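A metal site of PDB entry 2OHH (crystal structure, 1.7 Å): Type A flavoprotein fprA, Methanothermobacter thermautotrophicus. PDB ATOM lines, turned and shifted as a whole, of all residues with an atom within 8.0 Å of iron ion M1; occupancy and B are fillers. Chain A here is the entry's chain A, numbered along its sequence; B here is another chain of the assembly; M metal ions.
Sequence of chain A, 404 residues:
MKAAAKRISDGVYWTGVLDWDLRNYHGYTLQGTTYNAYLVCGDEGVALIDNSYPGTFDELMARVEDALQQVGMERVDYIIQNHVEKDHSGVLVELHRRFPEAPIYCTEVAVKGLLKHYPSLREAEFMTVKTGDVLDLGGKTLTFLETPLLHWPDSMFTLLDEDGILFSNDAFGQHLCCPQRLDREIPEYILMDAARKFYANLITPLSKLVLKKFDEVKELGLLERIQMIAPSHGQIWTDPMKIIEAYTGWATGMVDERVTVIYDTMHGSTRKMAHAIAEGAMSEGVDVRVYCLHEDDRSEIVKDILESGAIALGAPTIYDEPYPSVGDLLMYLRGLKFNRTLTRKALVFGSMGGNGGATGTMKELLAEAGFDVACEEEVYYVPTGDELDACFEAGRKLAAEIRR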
ATOM      1  N   TYR A  25      16.670   6.643  15.213  1.00  0.00           N
ATOM      2  CA  TYR A  25      16.855   5.287  14.758  1.00  0.00           C
ATOM      3  C   TYR A  25      18.303   4.885  15.024  1.00  0.00           C
ATOM      4  O   TYR A  25      19.212   5.464  14.478  1.00  0.00           O
ATOM      5  CB  TYR A  25      16.432   5.155  13.269  1.00  0.00           C
ATOM      6  CG  TYR A  25      16.451   3.721  12.801  1.00  0.00           C
ATOM      7  CD1 TYR A  25      15.854   2.716  13.583  1.00  0.00           C
ATOM      8  CD2 TYR A  25      17.099   3.357  11.605  1.00  0.00           C
ATOM      9  CE1 TYR A  25      15.888   1.384  13.195  1.00  0.00           C
ATOM     10  CE2 TYR A  25      17.144   2.026  11.208  1.00  0.00           C
ATOM     11  CZ  TYR A  25      16.527   1.039  12.011  1.00  0.00           C
ATOM     12  OH  TYR A  25      16.532  -0.298  11.657  1.00  0.00           O
ATOM     13  N   HIS A  26      18.499   3.920  15.920  1.00  0.00           N
ATOM     14  CA  HIS A  26      19.801   3.528  16.429  1.00  0.00           C
ATOM     15  C   HIS A  26      20.764   4.687  16.677  1.00  0.00           C
ATOM     16  O   HIS A  26      21.899   4.719  16.152  1.00  0.00           O
ATOM     17  CB  HIS A  26      20.405   2.397  15.605  1.00  0.00           C
ATOM     18  CG  HIS A  26      20.636   2.725  14.167  1.00  0.00           C
ATOM     19  ND1 HIS A  26      21.588   3.618  13.754  1.00  0.00           N
ATOM     20  CD2 HIS A  26      20.058   2.228  13.043  1.00  0.00           C
ATOM     21  CE1 HIS A  26      21.568   3.702  12.425  1.00  0.00           C
ATOM     22  NE2 HIS A  26      20.659   2.858  11.977  1.00  0.00           N
ATOM     23  N   THR A  33      11.695   8.479   8.003  1.00  0.00           N
ATOM     24  CA  THR A  33      12.500   7.838   7.030  1.00  0.00           C
ATOM     25  C   THR A  33      11.548   7.102   6.188  1.00  0.00           C
ATOM     26  O   THR A  33      10.336   7.203   6.358  1.00  0.00           O
ATOM     27  CB  THR A  33      13.530   6.874   7.600  1.00  0.00           C
ATOM     28  OG1 THR A  33      14.363   6.490   6.504  1.00  0.00           O
ATOM     29  CG2 THR A  33      12.865   5.637   8.188  1.00  0.00           C
ATOM     30  N   THR A  34      12.079   6.355   5.246  1.00  0.00           N
ATOM     31  CA  THR A  34      11.208   5.460   4.532  1.00  0.00           C
ATOM     32  C   THR A  34      11.831   4.072   4.536  1.00  0.00           C
ATOM     33  O   THR A  34      13.046   3.905   4.782  1.00  0.00           O
ATOM     34  CB  THR A  34      10.979   5.830   3.053  1.00  0.00           C
ATOM     35  OG1 THR A  34      12.143   5.563   2.299  1.00  0.00           O
ATOM     36  CG2 THR A  34      10.511   7.263   2.874  1.00  0.00           C
ATOM     37  N   TYR A  35      10.994   3.082   4.334  1.00  0.00           N
ATOM     38  CA  TYR A  35      11.478   1.701   4.140  1.00  0.00           C
ATOM     39  C   TYR A  35      11.085   1.366   2.737  1.00  0.00           C
ATOM     40  O   TYR A  35       9.874   1.163   2.430  1.00  0.00           O
ATOM     41  CB  TYR A  35      10.890   0.722   5.182  1.00  0.00           C
ATOM     42  CG  TYR A  35      10.969   1.292   6.568  1.00  0.00           C
ATOM     43  CD1 TYR A  35      12.216   1.612   7.131  1.00  0.00           C
ATOM     44  CD2 TYR A  35       9.823   1.566   7.286  1.00  0.00           C
ATOM     45  CE1 TYR A  35      12.306   2.165   8.378  1.00  0.00           C
ATOM     46  CE2 TYR A  35       9.904   2.137   8.546  1.00  0.00           C
ATOM     47  CZ  TYR A  35      11.148   2.404   9.075  1.00  0.00           C
ATOM     48  OH  TYR A  35      11.252   2.996  10.282  1.00  0.00           O
ATOM     49  N   ASN A  36      12.084   1.495   1.868  1.00  0.00           N
ATOM     50  CA  ASN A  36      11.769   1.308   0.411  1.00  0.00           C
ATOM     51  C   ASN A  36      11.832  -0.165   0.113  1.00  0.00           C
ATOM     52  O   ASN A  36      12.871  -0.856   0.347  1.00  0.00           O
ATOM     53  CB  ASN A  36      12.835   2.056  -0.429  1.00  0.00           C
ATOM     54  CG  ASN A  36      12.790   3.519  -0.181  1.00  0.00           C
ATOM     55  OD1 ASN A  36      11.726   4.070   0.145  1.00  0.00           O
ATOM     56  ND2 ASN A  36      13.908   4.178  -0.379  1.00  0.00           N
ATOM     57  N   ASP A  50      13.135  -6.299  -0.743  1.00  0.00           N
ATOM     58  CA  ASP A  50      13.082  -5.789   0.621  1.00  0.00           C
ATOM     59  C   ASP A  50      11.669  -5.619   1.118  1.00  0.00           C
ATOM     60  O   ASP A  50      10.677  -5.829   0.396  1.00  0.00           O
ATOM     61  CB  ASP A  50      13.916  -4.534   0.767  1.00  0.00           C
ATOM     62  CG  ASP A  50      15.415  -4.861   0.715  1.00  0.00           C
ATOM     63  OD1 ASP A  50      15.735  -6.048   0.990  1.00  0.00           O
ATOM     64  OD2 ASP A  50      16.208  -3.967   0.382  1.00  0.00           O
ATOM     65  N   HIS A  83      18.906  -7.546   2.823  1.00  0.00           N
ATOM     66  CA  HIS A  83      19.495  -7.290   4.147  1.00  0.00           C
ATOM     67  C   HIS A  83      18.490  -7.708   5.212  1.00  0.00           C
ATOM     68  O   HIS A  83      17.303  -7.739   4.949  1.00  0.00           O
ATOM     69  CB  HIS A  83      19.865  -5.804   4.126  1.00  0.00           C
ATOM     70  CG  HIS A  83      20.264  -5.213   5.420  1.00  0.00           C
ATOM     71  ND1 HIS A  83      21.259  -5.734   6.229  1.00  0.00           N
ATOM     72  CD2 HIS A  83      19.873  -4.059   6.003  1.00  0.00           C
ATOM     73  CE1 HIS A  83      21.407  -4.951   7.279  1.00  0.00           C
ATOM     74  NE2 HIS A  83      20.585  -3.923   7.160  1.00  0.00           N
ATOM     75  N   GLU A  85      18.154  -6.645   8.505  1.00  0.00           N
ATOM     76  CA  GLU A  85      17.780  -5.728   9.553  1.00  0.00           C
ATOM     77  C   GLU A  85      16.295  -5.554   9.542  1.00  0.00           C
ATOM     78  O   GLU A  85      15.656  -5.581   8.489  1.00  0.00           O
ATOM     79  CB  GLU A  85      18.473  -4.398   9.359  1.00  0.00           C
ATOM     80  CG  GLU A  85      18.556  -3.636  10.684  1.00  0.00           C
ATOM     81  CD  GLU A  85      19.356  -2.353  10.535  1.00  0.00           C
ATOM     82  OE1 GLU A  85      19.265  -1.491  11.445  1.00  0.00           O
ATOM     83  OE2 GLU A  85      20.086  -2.211   9.514  1.00  0.00           O
ATOM     84  N   LYS A  86      15.726  -5.349  10.709  1.00  0.00           N
ATOM     85  CA  LYS A  86      14.261  -5.466  10.805  1.00  0.00           C
ATOM     86  C   LYS A  86      13.489  -4.323  10.134  1.00  0.00           C
ATOM     87  O   LYS A  86      12.300  -4.469   9.876  1.00  0.00           O
ATOM     88  CB  LYS A  86      13.897  -5.587  12.281  1.00  0.00           C
ATOM     89  CG  LYS A  86      14.154  -4.316  12.994  1.00  0.00           C
ATOM     90  CD  LYS A  86      13.948  -4.437  14.505  1.00  0.00           C
ATOM     91  CE  LYS A  86      12.525  -4.692  14.915  1.00  0.00           C
ATOM     92  NZ  LYS A  86      12.479  -4.931  16.393  1.00  0.00           N
ATOM     93  N   ASP A  87      14.147  -3.212   9.799  1.00  0.00           N
ATOM     94  CA  ASP A  87      13.447  -2.176   9.016  1.00  0.00           C
ATOM     95  C   ASP A  87      13.208  -2.598   7.586  1.00  0.00           C
ATOM     96  O   ASP A  87      12.455  -1.957   6.869  1.00  0.00           O
ATOM     97  CB  ASP A  87      14.123  -0.796   9.082  1.00  0.00           C
ATOM     98  CG  ASP A  87      15.626  -0.815   8.806  1.00  0.00           C
ATOM     99  OD1 ASP A  87      16.321  -1.889   8.845  1.00  0.00           O
ATOM    100  OD2 ASP A  87      16.173   0.295   8.572  1.00  0.00           O
ATOM    101  N   HIS A  88      13.846  -3.694   7.177  1.00  0.00           N
ATOM    102  CA  HIS A  88      13.739  -4.173   5.816  1.00  0.00           C
ATOM    103  C   HIS A  88      13.223  -5.578   5.760  1.00  0.00           C
ATOM    104  O   HIS A  88      12.852  -6.014   4.696  1.00  0.00           O
ATOM    105  CB  HIS A  88      15.113  -4.070   5.130  1.00  0.00           C
ATOM    106  CG  HIS A  88      15.689  -2.694   5.225  1.00  0.00           C
ATOM    107  ND1 HIS A  88      15.030  -1.574   4.701  1.00  0.00           N
ATOM    108  CD2 HIS A  88      16.808  -2.242   5.831  1.00  0.00           C
ATOM    109  CE1 HIS A  88      15.759  -0.503   5.013  1.00  0.00           C
ATOM    110  NE2 HIS A  88      16.839  -0.883   5.673  1.00  0.00           N
ATOM    111  N   HIS A 151      25.718  -2.781   4.531  1.00  0.00           N
ATOM    112  CA  HIS A 151      26.376  -2.498   5.793  1.00  0.00           C
ATOM    113  C   HIS A 151      26.495  -3.650   6.808  1.00  0.00           C
ATOM    114  O   HIS A 151      26.991  -3.449   7.909  1.00  0.00           O
ATOM    115  CB  HIS A 151      25.819  -1.196   6.414  1.00  0.00           C
ATOM    116  CG  HIS A 151      24.679  -1.382   7.375  1.00  0.00           C
ATOM    117  ND1 HIS A 151      24.713  -0.918   8.674  1.00  0.00           N
ATOM    118  CD2 HIS A 151      23.508  -2.050   7.233  1.00  0.00           C
ATOM    119  CE1 HIS A 151      23.608  -1.267   9.281  1.00  0.00           C
ATOM    120  NE2 HIS A 151      22.850  -1.957   8.439  1.00  0.00           N
ATOM    121  N   ASN A 169      20.124  -1.703  -1.185  1.00  0.00           N
ATOM    122  CA  ASN A 169      19.935  -1.851   0.261  1.00  0.00           C
ATOM    123  C   ASN A 169      20.215  -0.480   0.897  1.00  0.00           C
ATOM    124  O   ASN A 169      19.892   0.565   0.326  1.00  0.00           O
ATOM    125  CB  ASN A 169      20.727  -3.100   0.891  1.00  0.00           C
ATOM    126  CG  ASN A 169      22.341  -2.969   1.063  1.00  0.00           C
ATOM    127  OD1 ASN A 169      22.894  -2.115   1.780  1.00  0.00           O
ATOM    128  ND2 ASN A 169      23.063  -3.921   0.453  1.00  0.00           N
ATOM    129  N   ASP A 170      20.808  -0.468   2.072  1.00  0.00           N
ATOM    130  CA  ASP A 170      21.051   0.786   2.736  1.00  0.00           C
ATOM    131  C   ASP A 170      22.059   1.694   2.035  1.00  0.00           C
ATOM    132  O   ASP A 170      21.977   2.915   2.188  1.00  0.00           O
ATOM    133  CB  ASP A 170      21.485   0.542   4.185  1.00  0.00           C
ATOM    134  CG  ASP A 170      20.279   0.519   5.158  1.00  0.00           C
ATOM    135  OD1 ASP A 170      19.137   0.240   4.744  1.00  0.00           O
ATOM    136  OD2 ASP A 170      20.469   0.787   6.364  1.00  0.00           O
ATOM    137  N   ALA A 171      22.984   1.120   1.263  1.00  0.00           N
ATOM    138  CA  ALA A 171      23.972   1.925   0.565  1.00  0.00           C
ATOM    139  C   ALA A 171      23.274   2.950  -0.294  1.00  0.00           C
ATOM    140  O   ALA A 171      22.313   2.618  -0.963  1.00  0.00           O
ATOM    141  CB  ALA A 171      24.835   1.093  -0.301  1.00  0.00           C
ATOM    142  N   GLY A 173      21.505   5.160   0.638  1.00  0.00           N
ATOM    143  CA  GLY A 173      20.256   5.537   1.293  1.00  0.00           C
ATOM    144  C   GLY A 173      20.324   6.919   1.915  1.00  0.00           C
ATOM    145  O   GLY A 173      21.425   7.471   2.099  1.00  0.00           O
ATOM    146  N   HIS A 175      17.948   9.062   5.131  1.00  0.00           N
ATOM    147  CA  HIS A 175      16.755   8.993   5.992  1.00  0.00           C
ATOM    148  C   HIS A 175      15.996  10.226   5.733  1.00  0.00           C
ATOM    149  O   HIS A 175      16.244  11.284   6.344  1.00  0.00           O
ATOM    150  CB  HIS A 175      17.161   8.805   7.479  1.00  0.00           C
ATOM    151  CG  HIS A 175      17.605   7.400   7.764  1.00  0.00           C
ATOM    152  ND1 HIS A 175      16.854   6.305   7.441  1.00  0.00           N
ATOM    153  CD2 HIS A 175      18.753   6.920   8.291  1.00  0.00           C
ATOM    154  CE1 HIS A 175      17.489   5.205   7.776  1.00  0.00           C
ATOM    155  NE2 HIS A 175      18.654   5.563   8.318  1.00  0.00           N
ATOM    156  N   PHE A 198      23.919  10.026   6.272  1.00  0.00           N
ATOM    157  CA  PHE A 198      23.791   8.624   6.241  1.00  0.00           C
ATOM    158  C   PHE A 198      25.135   8.009   6.015  1.00  0.00           C
ATOM    159  O   PHE A 198      25.497   7.065   6.701  1.00  0.00           O
ATOM    160  CB  PHE A 198      22.920   8.272   5.115  1.00  0.00           C
ATOM    161  CG  PHE A 198      22.423   6.869   5.126  1.00  0.00           C
ATOM    162  CD1 PHE A 198      21.127   6.593   5.549  1.00  0.00           C
ATOM    163  CD2 PHE A 198      23.184   5.842   4.624  1.00  0.00           C
ATOM    164  CE1 PHE A 198      20.599   5.295   5.493  1.00  0.00           C
ATOM    165  CE2 PHE A 198      22.702   4.532   4.586  1.00  0.00           C
ATOM    166  CZ  PHE A 198      21.404   4.255   5.019  1.00  0.00           C
ATOM    167  N   LEU A 202      26.695   5.639   8.936  1.00  0.00           N
ATOM    168  CA  LEU A 202      26.535   4.214   8.609  1.00  0.00           C
ATOM    169  C   LEU A 202      27.623   3.688   7.726  1.00  0.00           C
ATOM    170  O   LEU A 202      27.881   2.487   7.764  1.00  0.00           O
ATOM    171  CB  LEU A 202      25.207   3.983   7.901  1.00  0.00           C
ATOM    172  CG  LEU A 202      24.096   4.201   8.939  1.00  0.00           C
ATOM    173  CD1 LEU A 202      22.718   4.317   8.288  1.00  0.00           C
ATOM    174  CD2 LEU A 202      24.184   3.077   9.985  1.00  0.00           C
ATOM    175  N   PRO A 231      17.734   2.850  -3.200  1.00  0.00           N
ATOM    176  CA  PRO A 231      18.186   2.357  -1.929  1.00  0.00           C
ATOM    177  C   PRO A 231      17.005   2.005  -1.025  1.00  0.00           C
ATOM    178  O   PRO A 231      15.828   2.207  -1.391  1.00  0.00           O
ATOM    179  CB  PRO A 231      18.970   3.540  -1.359  1.00  0.00           C
ATOM    180  CG  PRO A 231      18.265   4.741  -1.886  1.00  0.00           C
ATOM    181  CD  PRO A 231      17.618   4.313  -3.240  1.00  0.00           C
ATOM    182  N   SER A 232      17.315   1.509   0.171  1.00  0.00           N
ATOM    183  CA  SER A 232      16.283   1.028   1.090  1.00  0.00           C
ATOM    184  C   SER A 232      15.683   2.123   1.969  1.00  0.00           C
ATOM    185  O   SER A 232      14.646   1.909   2.622  1.00  0.00           O
ATOM    186  CB  SER A 232      16.833  -0.132   1.947  1.00  0.00           C
ATOM    187  OG  SER A 232      16.944  -1.292   1.133  1.00  0.00           O
ATOM    188  N   HIS A 233      16.320   3.294   1.979  1.00  0.00           N
ATOM    189  CA  HIS A 233      15.788   4.500   2.594  1.00  0.00           C
ATOM    190  C   HIS A 233      15.883   5.713   1.715  1.00  0.00           C
ATOM    191  O   HIS A 233      16.895   5.936   1.037  1.00  0.00           O
ATOM    192  CB  HIS A 233      16.539   4.840   3.911  1.00  0.00           C
ATOM    193  CG  HIS A 233      16.570   3.714   4.870  1.00  0.00           C
ATOM    194  ND1 HIS A 233      15.465   3.322   5.603  1.00  0.00           N
ATOM    195  CD2 HIS A 233      17.545   2.824   5.139  1.00  0.00           C
ATOM    196  CE1 HIS A 233      15.788   2.258   6.327  1.00  0.00           C
ATOM    197  NE2 HIS A 233      17.049   1.962   6.081  1.00  0.00           N
ATOM    198  N   HIS B 267      17.314  -2.410  18.524  1.00  0.00           N
ATOM    199  CA  HIS B 267      16.153  -3.143  17.981  1.00  0.00           C
ATOM    200  C   HIS B 267      15.405  -3.941  19.007  1.00  0.00           C
ATOM    201  O   HIS B 267      14.443  -4.638  18.707  1.00  0.00           O
ATOM    202  CB  HIS B 267      16.579  -4.079  16.857  1.00  0.00           C
ATOM    203  CG  HIS B 267      17.087  -3.360  15.654  1.00  0.00           C
ATOM    204  ND1 HIS B 267      18.307  -3.648  15.076  1.00  0.00           N
ATOM    205  CD2 HIS B 267      16.568  -2.327  14.953  1.00  0.00           C
ATOM    206  CE1 HIS B 267      18.489  -2.844  14.039  1.00  0.00           C
ATOM    207  NE2 HIS B 267      17.437  -2.048  13.931  1.00  0.00           N
HETATM  208 FE    FE M   1      18.042   0.263   6.571  1.00  0.00          FE
HETATM  209 FE    FE M   2      20.785  -1.766   7.777  1.00  0.00          FE
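The side-chain carboxylate (OD2) of Asp 87 sits close to the side-chain hydroxyl (OH) of Tyr 25, at 3.2 Å.
A ring nitrogen (NE2) of His 88 lies close to the side-chain carboxylate (OD2) of Asp 87.
A ring nitrogen (NE2) of His 233 sits close to the side-chain carboxylate (OD2) of Asp 87, at 3.1 Å.
The backbone NH (N) of His 233 lies close to the side-chain amide nitrogen (ND2) of Asn 36 (3.5 Å).
ND1 of His 233 is in hydrogen-bond range of O of Thr 34 (2.6 Å).
A ring nitrogen (ND1) of His 233 sits at hydrogen-bond distance from the side-chain hydroxyl (OG1) of Thr 33 (3.5 Å).
The nearest printed residue that does not touch iron ion M1 is Glu 85 (4.4 Å).
NE2 of His 88 binds iron ion M1.
NE2 of His 233 is bound to iron ion M1 (2.0 Å).
The side-chain carboxylate (OD1) of Asp 170 binds iron ion M1, at 2.1 Å.
Iron ion M1 is bound by OD2 of Asp 170 (2.5 Å).
Slightly farther from iron ion M1 lies OD2 of Asp 87 (2.7 Å).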
